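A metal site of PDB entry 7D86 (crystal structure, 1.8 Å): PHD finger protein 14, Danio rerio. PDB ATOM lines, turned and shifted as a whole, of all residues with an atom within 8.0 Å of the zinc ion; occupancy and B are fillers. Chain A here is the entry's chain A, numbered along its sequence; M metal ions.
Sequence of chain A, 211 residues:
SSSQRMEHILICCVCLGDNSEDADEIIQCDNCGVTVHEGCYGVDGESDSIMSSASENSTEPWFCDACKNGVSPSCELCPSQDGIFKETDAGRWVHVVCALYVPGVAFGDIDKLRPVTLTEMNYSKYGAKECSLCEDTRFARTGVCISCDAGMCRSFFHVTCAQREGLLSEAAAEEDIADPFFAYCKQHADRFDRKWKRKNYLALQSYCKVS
The zinc ion is bound by the side-chain sulfur (SG) of Cys 32 (2.3 Å), the side-chain sulfur (SG) of Cys 29 (2.4 Å), the side-chain sulfur (SG) of Cys 67 (2.4 Å) and the side-chain sulfur (SG) of Cys 64 (2.5 Å).
The side-chain sulfur of Cys 67 lies close to the side-chain amide nitrogen of Asn 31 (3.3 Å).
The side-chain sulfur (SG) of Cys 32 lies close to the backbone NH (N) of Val 34, 3.6 Å away.
The side-chain sulfur (SG) of Cys 29 lies close to the backbone NH (N) of Asn 31 (3.4 Å).
The backbone NH (N) of Ala 66 lies close to the side-chain sulfur (SG) of Cys 64, at 3.6 Å.
N of Cys 29 lies within hydrogen-bond range of O of Val 34 (2.7 Å).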
ATOM      1  N   GLN A  28     -23.044  -2.812  23.866  1.00  0.00           N
ATOM      2  CA  GLN A  28     -21.732  -2.488  23.341  1.00  0.00           C
ATOM      3  C   GLN A  28     -20.968  -1.681  24.377  1.00  0.00           C
ATOM      4  O   GLN A  28     -21.507  -0.747  24.976  1.00  0.00           O
ATOM      5  CB  GLN A  28     -21.836  -1.704  22.030  1.00  0.00           C
ATOM      6  CG  GLN A  28     -20.503  -1.302  21.435  1.00  0.00           C
ATOM      7  CD  GLN A  28     -20.653  -0.744  20.034  1.00  0.00           C
ATOM      8  OE1 GLN A  28     -21.562   0.052  19.769  1.00  0.00           O
ATOM      9  NE2 GLN A  28     -19.780  -1.166  19.124  1.00  0.00           N
ATOM     10  N   CYS A  29     -19.708  -2.036  24.579  1.00  0.00           N
ATOM     11  CA  CYS A  29     -18.882  -1.290  25.524  1.00  0.00           C
ATOM     12  C   CYS A  29     -18.592   0.086  24.945  1.00  0.00           C
ATOM     13  O   CYS A  29     -18.096   0.207  23.826  1.00  0.00           O
ATOM     14  CB  CYS A  29     -17.582  -2.026  25.819  1.00  0.00           C
ATOM     15  SG  CYS A  29     -16.527  -1.118  26.963  1.00  0.00           S
ATOM     16  N   ASP A  30     -18.894   1.129  25.727  1.00  0.00           N
ATOM     17  CA  ASP A  30     -18.672   2.481  25.223  1.00  0.00           C
ATOM     18  C   ASP A  30     -17.206   2.858  25.171  1.00  0.00           C
ATOM     19  O   ASP A  30     -16.847   3.839  24.503  1.00  0.00           O
ATOM     20  CB  ASP A  30     -19.474   3.469  26.070  1.00  0.00           C
ATOM     21  CG  ASP A  30     -20.924   3.525  25.640  1.00  0.00           C
ATOM     22  OD1 ASP A  30     -21.197   3.991  24.516  1.00  0.00           O
ATOM     23  OD2 ASP A  30     -21.793   3.076  26.415  1.00  0.00           O
ATOM     24  N   ASN A  31     -16.331   2.084  25.826  1.00  0.00           N
ATOM     25  CA  ASN A  31     -14.906   2.367  25.807  1.00  0.00           C
ATOM     26  C   ASN A  31     -14.186   1.645  24.670  1.00  0.00           C
ATOM     27  O   ASN A  31     -13.506   2.295  23.862  1.00  0.00           O
ATOM     28  CB  ASN A  31     -14.278   1.991  27.156  1.00  0.00           C
ATOM     29  CG  ASN A  31     -12.880   2.563  27.332  1.00  0.00           C
ATOM     30  OD1 ASN A  31     -12.725   3.762  27.478  1.00  0.00           O
ATOM     31  ND2 ASN A  31     -11.875   1.698  27.312  1.00  0.00           N
ATOM     32  N   CYS A  32     -14.322   0.325  24.582  1.00  0.00           N
ATOM     33  CA  CYS A  32     -13.594  -0.462  23.592  1.00  0.00           C
ATOM     34  C   CYS A  32     -14.451  -0.911  22.421  1.00  0.00           C
ATOM     35  O   CYS A  32     -13.905  -1.427  21.434  1.00  0.00           O
ATOM     36  CB  CYS A  32     -12.949  -1.686  24.262  1.00  0.00           C
ATOM     37  SG  CYS A  32     -14.117  -2.954  24.831  1.00  0.00           S
ATOM     38  N   GLY A  33     -15.768  -0.763  22.493  1.00  0.00           N
ATOM     39  CA  GLY A  33     -16.635  -1.126  21.393  1.00  0.00           C
ATOM     40  C   GLY A  33     -17.015  -2.590  21.306  1.00  0.00           C
ATOM     41  O   GLY A  33     -17.722  -2.986  20.373  1.00  0.00           O
ATOM     42  N   VAL A  34     -16.592  -3.430  22.263  1.00  0.00           N
ATOM     43  CA  VAL A  34     -16.943  -4.843  22.194  1.00  0.00           C
ATOM     44  C   VAL A  34     -18.452  -4.989  22.336  1.00  0.00           C
ATOM     45  O   VAL A  34     -19.118  -4.191  23.014  1.00  0.00           O
ATOM     46  CB  VAL A  34     -16.191  -5.634  23.276  1.00  0.00           C
ATOM     47  CG1 VAL A  34     -16.775  -5.377  24.662  1.00  0.00           C
ATOM     48  CG2 VAL A  34     -16.199  -7.133  22.948  1.00  0.00           C
ATOM     49  N   THR A  35     -19.005  -5.998  21.667  1.00  0.00           N
ATOM     50  CA  THR A  35     -20.455  -6.208  21.616  1.00  0.00           C
ATOM     51  C   THR A  35     -20.771  -7.605  22.106  1.00  0.00           C
ATOM     52  O   THR A  35     -20.071  -8.567  21.767  1.00  0.00           O
ATOM     53  CB  THR A  35     -20.986  -6.031  20.187  1.00  0.00           C
ATOM     54  OG1 THR A  35     -20.207  -6.817  19.289  1.00  0.00           O
ATOM     55  CG2 THR A  35     -20.903  -4.559  19.776  1.00  0.00           C
ATOM     56  N   TYR A  41     -23.171 -12.364  28.916  1.00  0.00           N
ATOM     57  CA  TYR A  41     -22.190 -11.691  29.769  1.00  0.00           C
ATOM     58  C   TYR A  41     -22.628 -11.598  31.222  1.00  0.00           C
ATOM     59  O   TYR A  41     -21.934 -10.963  32.023  1.00  0.00           O
ATOM     60  CB  TYR A  41     -21.909 -10.271  29.237  1.00  0.00           C
ATOM     61  CG  TYR A  41     -20.580  -9.695  29.675  1.00  0.00           C
ATOM     62  CD1 TYR A  41     -19.393 -10.365  29.414  1.00  0.00           C
ATOM     63  CD2 TYR A  41     -20.504  -8.452  30.315  1.00  0.00           C
ATOM     64  CE1 TYR A  41     -18.180  -9.848  29.791  1.00  0.00           C
ATOM     65  CE2 TYR A  41     -19.286  -7.922  30.703  1.00  0.00           C
ATOM     66  CZ  TYR A  41     -18.132  -8.622  30.427  1.00  0.00           C
ATOM     67  OH  TYR A  41     -16.910  -8.099  30.802  1.00  0.00           O
ATOM     68  N   TRP A  62     -22.144   2.143  29.193  1.00  0.00           N
ATOM     69  CA  TRP A  62     -21.842   0.850  29.790  1.00  0.00           C
ATOM     70  C   TRP A  62     -20.423   0.444  29.437  1.00  0.00           C
ATOM     71  O   TRP A  62     -20.010   0.570  28.275  1.00  0.00           O
ATOM     72  CB  TRP A  62     -22.827  -0.226  29.326  1.00  0.00           C
ATOM     73  CG  TRP A  62     -22.521  -1.591  29.875  1.00  0.00           C
ATOM     74  CD1 TRP A  62     -22.822  -2.061  31.117  1.00  0.00           C
ATOM     75  CD2 TRP A  62     -21.868  -2.661  29.187  1.00  0.00           C
ATOM     76  NE1 TRP A  62     -22.383  -3.347  31.261  1.00  0.00           N
ATOM     77  CE2 TRP A  62     -21.799  -3.749  30.089  1.00  0.00           C
ATOM     78  CE3 TRP A  62     -21.325  -2.812  27.911  1.00  0.00           C
ATOM     79  CZ2 TRP A  62     -21.206  -4.970  29.742  1.00  0.00           C
ATOM     80  CZ3 TRP A  62     -20.737  -4.025  27.566  1.00  0.00           C
ATOM     81  CH2 TRP A  62     -20.694  -5.086  28.487  1.00  0.00           C
ATOM     82  N   PHE A  63     -19.684  -0.044  30.424  1.00  0.00           N
ATOM     83  CA  PHE A  63     -18.322  -0.523  30.233  1.00  0.00           C
ATOM     84  C   PHE A  63     -18.283  -2.023  30.470  1.00  0.00           C
ATOM     85  O   PHE A  63     -18.971  -2.550  31.353  1.00  0.00           O
ATOM     86  CB  PHE A  63     -17.338   0.153  31.188  1.00  0.00           C
ATOM     87  CG  PHE A  63     -16.968   1.549  30.799  1.00  0.00           C
ATOM     88  CD1 PHE A  63     -17.538   2.157  29.702  1.00  0.00           C
ATOM     89  CD2 PHE A  63     -16.028   2.256  31.540  1.00  0.00           C
ATOM     90  CE1 PHE A  63     -17.186   3.461  29.350  1.00  0.00           C
ATOM     91  CE2 PHE A  63     -15.676   3.545  31.198  1.00  0.00           C
ATOM     92  CZ  PHE A  63     -16.257   4.149  30.093  1.00  0.00           C
ATOM     93  N   CYS A  64     -17.475  -2.717  29.676  1.00  0.00           N
ATOM     94  CA  CYS A  64     -17.182  -4.107  29.979  1.00  0.00           C
ATOM     95  C   CYS A  64     -16.310  -4.184  31.227  1.00  0.00           C
ATOM     96  O   CYS A  64     -15.752  -3.176  31.699  1.00  0.00           O
ATOM     97  CB  CYS A  64     -16.512  -4.802  28.794  1.00  0.00           C
ATOM     98  SG  CYS A  64     -14.755  -4.394  28.567  1.00  0.00           S
ATOM     99  N   ASP A  65     -16.197  -5.385  31.791  1.00  0.00           N
ATOM    100  CA  ASP A  65     -15.470  -5.554  33.043  1.00  0.00           C
ATOM    101  C   ASP A  65     -14.012  -5.166  32.912  1.00  0.00           C
ATOM    102  O   ASP A  65     -13.446  -4.581  33.841  1.00  0.00           O
ATOM    103  CB  ASP A  65     -15.596  -6.998  33.528  1.00  0.00           C
ATOM    104  CG  ASP A  65     -16.990  -7.333  34.029  1.00  0.00           C
ATOM    105  OD1 ASP A  65     -17.875  -6.455  33.951  1.00  0.00           O
ATOM    106  OD2 ASP A  65     -17.184  -8.466  34.494  1.00  0.00           O
ATOM    107  N   ALA A  66     -13.385  -5.463  31.770  1.00  0.00           N
ATOM    108  CA  ALA A  66     -11.985  -5.090  31.599  1.00  0.00           C
ATOM    109  C   ALA A  66     -11.814  -3.571  31.604  1.00  0.00           C
ATOM    110  O   ALA A  66     -10.920  -3.032  32.270  1.00  0.00           O
ATOM    111  CB  ALA A  66     -11.432  -5.691  30.315  1.00  0.00           C
ATOM    112  N   CYS A  67     -12.685  -2.854  30.892  1.00  0.00           N
ATOM    113  CA  CYS A  67     -12.572  -1.402  30.863  1.00  0.00           C
ATOM    114  C   CYS A  67     -12.943  -0.783  32.211  1.00  0.00           C
ATOM    115  O   CYS A  67     -12.406   0.262  32.567  1.00  0.00           O
ATOM    116  CB  CYS A  67     -13.434  -0.839  29.736  1.00  0.00           C
ATOM    117  SG  CYS A  67     -12.840  -1.336  28.101  1.00  0.00           S
ATOM    118  N   LYS A  68     -13.847  -1.420  32.968  1.00  0.00           N
ATOM    119  CA  LYS A  68     -14.131  -0.965  34.324  1.00  0.00           C
ATOM    120  C   LYS A  68     -12.897  -0.999  35.226  1.00  0.00           C
ATOM    121  O   LYS A  68     -12.849  -0.262  36.212  1.00  0.00           O
ATOM    122  CB  LYS A  68     -15.227  -1.817  34.963  1.00  0.00           C
ATOM    123  CG  LYS A  68     -16.648  -1.382  34.701  1.00  0.00           C
ATOM    124  CD  LYS A  68     -17.580  -2.149  35.638  1.00  0.00           C
ATOM    125  CE  LYS A  68     -19.048  -1.884  35.353  1.00  0.00           C
ATOM    126  NZ  LYS A  68     -19.887  -2.445  36.441  1.00  0.00           N
ATOM    127  N   VAL A  71      -8.003  -2.005  32.080  1.00  0.00           N
ATOM    128  CA  VAL A  71      -6.998  -2.910  31.543  1.00  0.00           C
ATOM    129  C   VAL A  71      -7.419  -3.358  30.151  1.00  0.00           C
ATOM    130  O   VAL A  71      -8.608  -3.477  29.843  1.00  0.00           O
ATOM    131  CB  VAL A  71      -6.765  -4.133  32.439  1.00  0.00           C
ATOM    132  CG1 VAL A  71      -5.947  -3.757  33.664  1.00  0.00           C
ATOM    133  CG2 VAL A  71      -8.083  -4.728  32.861  1.00  0.00           C
ATOM    134  N   SER A  72      -6.416  -3.593  29.310  1.00  0.00           N
ATOM    135  CA  SER A  72      -6.584  -4.405  28.108  1.00  0.00           C
ATOM    136  C   SER A  72      -5.947  -5.745  28.410  1.00  0.00           C
ATOM    137  O   SER A  72      -4.741  -5.917  28.238  1.00  0.00           O
ATOM    138  CB  SER A  72      -5.929  -3.750  26.884  1.00  0.00           C
ATOM    139  OG  SER A  72      -6.640  -2.594  26.492  1.00  0.00           O
ATOM    140  N   PRO A  73      -6.713  -6.712  28.883  1.00  0.00           N
ATOM    141  CA  PRO A  73      -6.122  -7.915  29.463  1.00  0.00           C
ATOM    142  C   PRO A  73      -5.703  -8.914  28.392  1.00  0.00           C
ATOM    143  O   PRO A  73      -6.059  -8.805  27.226  1.00  0.00           O
ATOM    144  CB  PRO A  73      -7.260  -8.469  30.321  1.00  0.00           C
ATOM    145  CG  PRO A  73      -8.485  -8.129  29.534  1.00  0.00           C
ATOM    146  CD  PRO A  73      -8.197  -6.793  28.860  1.00  0.00           C
ATOM    147  N   GLY A  83     -12.136  -9.912  21.796  1.00  0.00           N
ATOM    148  CA  GLY A  83     -13.241 -10.512  22.519  1.00  0.00           C
ATOM    149  C   GLY A  83     -13.455  -9.870  23.885  1.00  0.00           C
ATOM    150  O   GLY A  83     -12.879  -8.832  24.222  1.00  0.00           O
ATOM    151  N   ILE A  84     -14.299 -10.513  24.680  1.00  0.00           N
ATOM    152  CA  ILE A  84     -14.721  -9.932  25.943  1.00  0.00           C
ATOM    153  C   ILE A  84     -14.268 -10.841  27.083  1.00  0.00           C
ATOM    154  O   ILE A  84     -14.207 -12.072  26.937  1.00  0.00           O
ATOM    155  CB  ILE A  84     -16.246  -9.672  25.947  1.00  0.00           C
ATOM    156  CG1 ILE A  84     -16.580  -8.535  26.918  1.00  0.00           C
ATOM    157  CG2 ILE A  84     -17.042 -10.917  26.291  1.00  0.00           C
ATOM    158  CD1 ILE A  84     -18.000  -8.032  26.785  1.00  0.00           C
ATOM    159  N   PHE A  85     -13.914 -10.218  28.206  1.00  0.00           N
ATOM    160  CA  PHE A  85     -13.218 -10.867  29.302  1.00  0.00           C
ATOM    161  C   PHE A  85     -14.010 -10.758  30.600  1.00  0.00           C
ATOM    162  O   PHE A  85     -14.803  -9.836  30.802  1.00  0.00           O
ATOM    163  CB  PHE A  85     -11.839 -10.251  29.547  1.00  0.00           C
ATOM    164  CG  PHE A  85     -10.868 -10.455  28.428  1.00  0.00           C
ATOM    165  CD1 PHE A  85     -10.903  -9.656  27.298  1.00  0.00           C
ATOM    166  CD2 PHE A  85      -9.890 -11.448  28.527  1.00  0.00           C
ATOM    167  CE1 PHE A  85      -9.992  -9.837  26.277  1.00  0.00           C
ATOM    168  CE2 PHE A  85      -8.980 -11.629  27.506  1.00  0.00           C
ATOM    169  CZ  PHE A  85      -9.030 -10.826  26.370  1.00  0.00           C
HETATM  170 ZN    ZN M   1     -14.602  -2.499  27.013  1.00  0.00          ZN
